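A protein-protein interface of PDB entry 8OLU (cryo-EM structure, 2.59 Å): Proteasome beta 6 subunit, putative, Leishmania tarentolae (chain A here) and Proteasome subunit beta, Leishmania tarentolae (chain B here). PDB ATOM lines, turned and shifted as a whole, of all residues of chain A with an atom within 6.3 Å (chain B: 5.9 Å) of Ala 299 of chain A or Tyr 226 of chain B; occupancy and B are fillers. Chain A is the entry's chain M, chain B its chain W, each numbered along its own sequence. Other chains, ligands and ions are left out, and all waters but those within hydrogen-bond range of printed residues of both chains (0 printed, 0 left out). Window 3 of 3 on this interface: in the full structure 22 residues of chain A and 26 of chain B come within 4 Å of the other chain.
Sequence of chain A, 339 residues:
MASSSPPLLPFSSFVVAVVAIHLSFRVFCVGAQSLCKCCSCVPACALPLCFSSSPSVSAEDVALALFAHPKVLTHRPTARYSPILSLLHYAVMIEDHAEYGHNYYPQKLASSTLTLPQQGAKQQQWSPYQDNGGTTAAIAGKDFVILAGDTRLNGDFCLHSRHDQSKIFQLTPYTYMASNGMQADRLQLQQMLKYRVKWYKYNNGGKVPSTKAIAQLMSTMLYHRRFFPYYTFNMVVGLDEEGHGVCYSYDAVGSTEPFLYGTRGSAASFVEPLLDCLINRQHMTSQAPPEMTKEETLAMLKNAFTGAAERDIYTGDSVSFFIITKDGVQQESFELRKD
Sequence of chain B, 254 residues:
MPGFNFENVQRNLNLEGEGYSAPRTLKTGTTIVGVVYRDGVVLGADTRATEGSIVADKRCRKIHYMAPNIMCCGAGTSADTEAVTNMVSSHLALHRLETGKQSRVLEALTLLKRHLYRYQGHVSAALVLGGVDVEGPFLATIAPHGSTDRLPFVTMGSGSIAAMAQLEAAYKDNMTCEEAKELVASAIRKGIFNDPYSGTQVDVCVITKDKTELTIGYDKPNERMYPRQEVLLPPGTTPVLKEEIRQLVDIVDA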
ATOM      1  N   LYS A 294     -18.859  13.011   8.505  1.00  0.00           N
ATOM      2  CA  LYS A 294     -19.088  14.432   8.587  1.00  0.00           C
ATOM      3  C   LYS A 294     -19.860  14.758   9.852  1.00  0.00           C
ATOM      4  O   LYS A 294     -19.678  15.851  10.363  1.00  0.00           O
ATOM      5  CB  LYS A 294     -19.685  14.981   7.295  1.00  0.00           C
ATOM      6  CG  LYS A 294     -21.179  15.206   7.242  1.00  0.00           C
ATOM      7  CD  LYS A 294     -21.573  15.409   5.793  1.00  0.00           C
ATOM      8  CE  LYS A 294     -23.064  15.240   5.576  1.00  0.00           C
ATOM      9  NZ  LYS A 294     -23.344  14.957   4.151  1.00  0.00           N
ATOM     10  N   GLU A 295     -20.620  13.819  10.430  1.00  0.00           N
ATOM     11  CA  GLU A 295     -21.282  14.087  11.705  1.00  0.00           C
ATOM     12  C   GLU A 295     -20.243  14.092  12.830  1.00  0.00           C
ATOM     13  O   GLU A 295     -20.279  14.947  13.716  1.00  0.00           O
ATOM     14  CB  GLU A 295     -22.428  13.120  11.971  1.00  0.00           C
ATOM     15  CG  GLU A 295     -23.550  13.224  10.937  1.00  0.00           C
ATOM     16  CD  GLU A 295     -23.373  12.521   9.581  1.00  0.00           C
ATOM     17  OE1 GLU A 295     -22.287  11.906   9.319  1.00  0.00           O
ATOM     18  OE2 GLU A 295     -24.337  12.573   8.769  1.00  0.00           O
ATOM     19  N   GLU A 296     -19.297  13.168  12.768  1.00  0.00           N
ATOM     20  CA  GLU A 296     -18.322  13.063  13.825  1.00  0.00           C
ATOM     21  C   GLU A 296     -17.352  14.227  13.796  1.00  0.00           C
ATOM     22  O   GLU A 296     -16.794  14.592  14.821  1.00  0.00           O
ATOM     23  CB  GLU A 296     -17.483  11.802  13.681  1.00  0.00           C
ATOM     24  CG  GLU A 296     -18.260  10.527  13.987  1.00  0.00           C
ATOM     25  CD  GLU A 296     -17.412   9.265  13.909  1.00  0.00           C
ATOM     26  OE1 GLU A 296     -17.497   8.454  14.865  1.00  0.00           O
ATOM     27  OE2 GLU A 296     -16.657   9.097  12.905  1.00  0.00           O
ATOM     28  N   THR A 297     -17.095  14.731  12.590  1.00  0.00           N
ATOM     29  CA  THR A 297     -16.161  15.815  12.392  1.00  0.00           C
ATOM     30  C   THR A 297     -16.779  17.054  12.984  1.00  0.00           C
ATOM     31  O   THR A 297     -16.130  17.829  13.664  1.00  0.00           O
ATOM     32  CB  THR A 297     -15.928  16.088  10.909  1.00  0.00           C
ATOM     33  OG1 THR A 297     -15.482  14.880  10.297  1.00  0.00           O
ATOM     34  CG2 THR A 297     -14.902  17.170  10.640  1.00  0.00           C
ATOM     35  N   LEU A 298     -18.056  17.216  12.687  1.00  0.00           N
ATOM     36  CA  LEU A 298     -18.798  18.351  13.178  1.00  0.00           C
ATOM     37  C   LEU A 298     -18.821  18.340  14.695  1.00  0.00           C
ATOM     38  O   LEU A 298     -18.397  19.309  15.293  1.00  0.00           O
ATOM     39  CB  LEU A 298     -20.184  18.305  12.553  1.00  0.00           C
ATOM     40  CG  LEU A 298     -21.151  19.355  13.060  1.00  0.00           C
ATOM     41  CD1 LEU A 298     -20.649  20.728  12.718  1.00  0.00           C
ATOM     42  CD2 LEU A 298     -22.519  19.130  12.437  1.00  0.00           C
ATOM     43  N   ALA A 299     -19.204  17.238  15.323  1.00  0.00           N
ATOM     44  CA  ALA A 299     -19.079  17.128  16.765  1.00  0.00           C
ATOM     45  C   ALA A 299     -17.705  17.583  17.216  1.00  0.00           C
ATOM     46  O   ALA A 299     -17.593  18.343  18.154  1.00  0.00           O
ATOM     47  CB  ALA A 299     -19.324  15.740  17.251  1.00  0.00           C
ATOM     48  N   MET A 300     -16.667  17.142  16.544  1.00  0.00           N
ATOM     49  CA  MET A 300     -15.338  17.463  17.008  1.00  0.00           C
ATOM     50  C   MET A 300     -15.130  18.986  17.042  1.00  0.00           C
ATOM     51  O   MET A 300     -14.563  19.516  17.983  1.00  0.00           O
ATOM     52  CB  MET A 300     -14.276  16.779  16.147  1.00  0.00           C
ATOM     53  CG  MET A 300     -12.899  17.321  16.410  1.00  0.00           C
ATOM     54  SD  MET A 300     -11.603  16.442  15.546  1.00  0.00           S
ATOM     55  CE  MET A 300     -11.774  14.866  16.394  1.00  0.00           C
ATOM     56  N   LEU A 301     -15.576  19.699  16.029  1.00  0.00           N
ATOM     57  CA  LEU A 301     -15.431  21.132  15.982  1.00  0.00           C
ATOM     58  C   LEU A 301     -16.347  21.829  16.970  1.00  0.00           C
ATOM     59  O   LEU A 301     -16.024  22.937  17.405  1.00  0.00           O
ATOM     60  CB  LEU A 301     -15.868  21.626  14.621  1.00  0.00           C
ATOM     61  CG  LEU A 301     -14.796  21.642  13.547  1.00  0.00           C
ATOM     62  CD1 LEU A 301     -15.377  22.245  12.291  1.00  0.00           C
ATOM     63  CD2 LEU A 301     -13.600  22.439  13.966  1.00  0.00           C
ATOM     64  N   LYS A 302     -17.524  21.258  17.250  1.00  0.00           N
ATOM     65  CA  LYS A 302     -18.325  21.808  18.314  1.00  0.00           C
ATOM     66  C   LYS A 302     -17.597  21.663  19.634  1.00  0.00           C
ATOM     67  O   LYS A 302     -17.646  22.550  20.469  1.00  0.00           O
ATOM     68  CB  LYS A 302     -19.660  21.109  18.443  1.00  0.00           C
ATOM     69  CG  LYS A 302     -20.639  21.519  17.369  1.00  0.00           C
ATOM     70  CD  LYS A 302     -21.941  20.769  17.434  1.00  0.00           C
ATOM     71  CE  LYS A 302     -22.772  21.046  16.201  1.00  0.00           C
ATOM     72  NZ  LYS A 302     -24.188  20.690  16.421  1.00  0.00           N
ATOM     73  N   ASN A 303     -16.976  20.531  19.866  1.00  0.00           N
ATOM     74  CA  ASN A 303     -16.370  20.330  21.157  1.00  0.00           C
ATOM     75  C   ASN A 303     -15.228  21.336  21.288  1.00  0.00           C
ATOM     76  O   ASN A 303     -14.917  21.797  22.391  1.00  0.00           O
ATOM     77  CB  ASN A 303     -15.930  18.894  21.374  1.00  0.00           C
ATOM     78  CG  ASN A 303     -15.236  18.740  22.716  1.00  0.00           C
ATOM     79  OD1 ASN A 303     -15.901  18.814  23.747  1.00  0.00           O
ATOM     80  ND2 ASN A 303     -13.913  18.567  22.742  1.00  0.00           N
ATOM     81  N   ALA A 304     -14.614  21.718  20.178  1.00  0.00           N
ATOM     82  CA  ALA A 304     -13.368  22.457  20.284  1.00  0.00           C
ATOM     83  C   ALA A 304     -13.636  23.968  20.268  1.00  0.00           C
ATOM     84  O   ALA A 304     -12.954  24.726  20.950  1.00  0.00           O
ATOM     85  CB  ALA A 304     -12.423  22.051  19.184  1.00  0.00           C
ATOM     86  N   THR A 306     -16.357  24.868  21.663  1.00  0.00           N
ATOM     87  CA  THR A 306     -16.970  25.016  22.960  1.00  0.00           C
ATOM     88  C   THR A 306     -15.917  25.293  24.011  1.00  0.00           C
ATOM     89  O   THR A 306     -16.056  26.281  24.706  1.00  0.00           O
ATOM     90  CB  THR A 306     -17.796  23.797  23.332  1.00  0.00           C
ATOM     91  OG1 THR A 306     -18.970  23.868  22.522  1.00  0.00           O
ATOM     92  CG2 THR A 306     -18.127  23.836  24.793  1.00  0.00           C
ATOM     93  N   PHE A 334     -24.718  27.202  16.160  1.00  0.00           N
ATOM     94  CA  PHE A 334     -24.394  26.478  17.358  1.00  0.00           C
ATOM     95  C   PHE A 334     -24.051  27.450  18.479  1.00  0.00           C
ATOM     96  O   PHE A 334     -23.117  28.222  18.321  1.00  0.00           O
ATOM     97  CB  PHE A 334     -23.186  25.637  16.997  1.00  0.00           C
ATOM     98  CG  PHE A 334     -22.694  24.873  18.176  1.00  0.00           C
ATOM     99  CD1 PHE A 334     -23.560  24.023  18.844  1.00  0.00           C
ATOM    100  CD2 PHE A 334     -21.400  25.047  18.624  1.00  0.00           C
ATOM    101  CE1 PHE A 334     -23.105  23.311  19.939  1.00  0.00           C
ATOM    102  CE2 PHE A 334     -20.948  24.334  19.729  1.00  0.00           C
ATOM    103  CZ  PHE A 334     -21.795  23.458  20.365  1.00  0.00           C
ATOM    104  N   GLU A 335     -24.789  27.412  19.588  1.00  0.00           N
ATOM    105  CA  GLU A 335     -24.581  28.411  20.625  1.00  0.00           C
ATOM    106  C   GLU A 335     -23.322  28.087  21.435  1.00  0.00           C
ATOM    107  O   GLU A 335     -23.024  26.934  21.737  1.00  0.00           O
ATOM    108  CB  GLU A 335     -25.837  28.584  21.487  1.00  0.00           C
ATOM    109  CG  GLU A 335     -27.103  28.963  20.696  1.00  0.00           C
ATOM    110  CD  GLU A 335     -27.106  30.268  19.883  1.00  0.00           C
ATOM    111  OE1 GLU A 335     -27.262  31.360  20.498  1.00  0.00           O
ATOM    112  OE2 GLU A 335     -26.953  30.203  18.612  1.00  0.00           O
ATOM    113  N   ARG B 224     -22.543  25.328  30.581  1.00  0.00           N
ATOM    114  CA  ARG B 224     -22.010  25.087  29.240  1.00  0.00           C
ATOM    115  C   ARG B 224     -23.055  24.325  28.414  1.00  0.00           C
ATOM    116  O   ARG B 224     -23.781  23.478  28.934  1.00  0.00           O
ATOM    117  CB  ARG B 224     -20.622  24.426  29.272  1.00  0.00           C
ATOM    118  CG  ARG B 224     -20.557  23.001  29.809  1.00  0.00           C
ATOM    119  CD  ARG B 224     -19.140  22.453  29.675  1.00  0.00           C
ATOM    120  NE  ARG B 224     -18.717  22.242  28.290  1.00  0.00           N
ATOM    121  CZ  ARG B 224     -17.465  21.997  27.894  1.00  0.00           C
ATOM    122  NH1 ARG B 224     -17.229  21.160  26.897  1.00  0.00           N
ATOM    123  NH2 ARG B 224     -16.442  22.565  28.507  1.00  0.00           N
ATOM    124  N   MET B 225     -23.116  24.643  27.110  1.00  0.00           N
ATOM    125  CA  MET B 225     -24.312  24.454  26.297  1.00  0.00           C
ATOM    126  C   MET B 225     -24.232  23.169  25.459  1.00  0.00           C
ATOM    127  O   MET B 225     -25.262  22.652  25.019  1.00  0.00           O
ATOM    128  CB  MET B 225     -24.497  25.690  25.403  1.00  0.00           C
ATOM    129  CG  MET B 225     -24.714  26.978  26.212  1.00  0.00           C
ATOM    130  SD  MET B 225     -24.710  28.538  25.268  1.00  0.00           S
ATOM    131  CE  MET B 225     -26.470  28.841  25.072  1.00  0.00           C
ATOM    132  N   TYR B 226     -23.002  22.668  25.236  1.00  0.00           N
ATOM    133  CA  TYR B 226     -22.722  21.345  24.681  1.00  0.00           C
ATOM    134  C   TYR B 226     -22.136  20.483  25.810  1.00  0.00           C
ATOM    135  O   TYR B 226     -21.122  20.878  26.386  1.00  0.00           O
ATOM    136  CB  TYR B 226     -21.746  21.507  23.498  1.00  0.00           C
ATOM    137  CG  TYR B 226     -21.649  20.395  22.465  1.00  0.00           C
ATOM    138  CD1 TYR B 226     -22.760  19.962  21.740  1.00  0.00           C
ATOM    139  CD2 TYR B 226     -20.422  19.804  22.161  1.00  0.00           C
ATOM    140  CE1 TYR B 226     -22.663  18.958  20.783  1.00  0.00           C
ATOM    141  CE2 TYR B 226     -20.307  18.795  21.210  1.00  0.00           C
ATOM    142  CZ  TYR B 226     -21.432  18.369  20.514  1.00  0.00           C
ATOM    143  OH  TYR B 226     -21.325  17.370  19.558  1.00  0.00           O
ATOM    144  N   PRO B 227     -22.702  19.304  26.202  1.00  0.00           N
ATOM    145  CA  PRO B 227     -22.066  18.500  27.253  1.00  0.00           C
ATOM    146  C   PRO B 227     -20.688  18.045  26.765  1.00  0.00           C
ATOM    147  O   PRO B 227     -20.508  17.751  25.586  1.00  0.00           O
ATOM    148  CB  PRO B 227     -23.048  17.350  27.564  1.00  0.00           C
ATOM    149  CG  PRO B 227     -24.053  17.346  26.399  1.00  0.00           C
ATOM    150  CD  PRO B 227     -23.939  18.684  25.684  1.00  0.00           C
ATOM    151  N   ARG B 228     -19.712  18.033  27.684  1.00  0.00           N
ATOM    152  CA  ARG B 228     -18.337  17.666  27.375  1.00  0.00           C
ATOM    153  C   ARG B 228     -18.350  16.294  26.696  1.00  0.00           C
ATOM    154  O   ARG B 228     -19.172  15.446  27.039  1.00  0.00           O
ATOM    155  CB  ARG B 228     -17.481  17.696  28.652  1.00  0.00           C
ATOM    156  CG  ARG B 228     -15.972  17.733  28.421  1.00  0.00           C
ATOM    157  CD  ARG B 228     -15.147  17.998  29.676  1.00  0.00           C
ATOM    158  NE  ARG B 228     -15.349  19.319  30.292  1.00  0.00           N
ATOM    159  CZ  ARG B 228     -15.708  19.547  31.561  1.00  0.00           C
ATOM    160  NH1 ARG B 228     -15.450  20.712  32.133  1.00  0.00           N
ATOM    161  NH2 ARG B 228     -16.304  18.603  32.268  1.00  0.00           N
ATOM    162  N   GLN B 229     -17.468  16.110  25.701  1.00  0.00           N
ATOM    163  CA  GLN B 229     -17.380  14.870  24.944  1.00  0.00           C
ATOM    164  C   GLN B 229     -16.192  14.071  25.465  1.00  0.00           C
ATOM    165  O   GLN B 229     -15.052  14.371  25.131  1.00  0.00           O
ATOM    166  CB  GLN B 229     -17.196  15.124  23.441  1.00  0.00           C
ATOM    167  CG  GLN B 229     -18.350  15.858  22.762  1.00  0.00           C
ATOM    168  CD  GLN B 229     -19.655  15.092  22.777  1.00  0.00           C
ATOM    169  OE1 GLN B 229     -19.799  14.055  22.133  1.00  0.00           O
ATOM    170  NE2 GLN B 229     -20.629  15.623  23.501  1.00  0.00           N
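Of the 6 printed residues of chain B, 4 touch a printed residue of chain A.
Hydrophobic or aromatic side chains of chain A that line the printed part of chain B: Ala 299 and Phe 334.
Along chain A the printed residues that touch a printed residue of chain B span positions 299 to 335.
The guanidinium group (NE) of Arg 224 of chain B is in hydrogen-bond range of the backbone carbonyl oxygen (O) of Tyr 226 of chain B, at 3.4 Å.
The backbone carbonyl oxygen (O) of Pro 227 of chain B lies within hydrogen-bond range of the side-chain amide nitrogen (NE2) of Gln 229 of chain B (3.0 Å).
O of Lys 302 of chain A sits at hydrogen-bond distance from OG1 of Thr 306 of chain A.
Among the printed residues, pairs that only touch across the chains: Ala 299 of chain A with Tyr 226 of chain B (3.5 Å), Thr 306 of chain A with Arg 224 of chain B (3.5 Å), Glu 335 of chain A with Met 225 of chain B (3.6 Å), Lys 302 of chain A with Tyr 226 of chain B (3.7 Å), Asn 303 of chain A with Gln 229 of chain B (3.7 Å), Phe 334 of chain A with Tyr 226 of chain B (3.7 Å), Thr 306 of chain A with Tyr 226 of chain B (3.8 Å) and Asn 303 of chain A with Tyr 226 of chain B (3.99 Å).
Glu 295 of chain A touches none of the printed residues of chain B.
Printed residues of chain B within 4 Å of Lys 302 of chain A: Tyr 226 (3.7 Å).
Ala 304 of chain A touches none of the printed residues of chain B.
Printed residues of chain A within 4 Å of Tyr 226 of chain B: Ala 299, Lys 302, Asn 303, Thr 306 and Phe 334.
Of the printed residues of chain A, Gln 229 of chain B touches Asn 303 (3.7 Å).
The nearest residue of chain B that does not touch Ala 299 of chain A is Gln 229 of chain B (5.2 Å).
The nearest printed residue of chain A that does not touch Tyr 226 of chain B is Glu 335 of chain A (5.5 Å).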
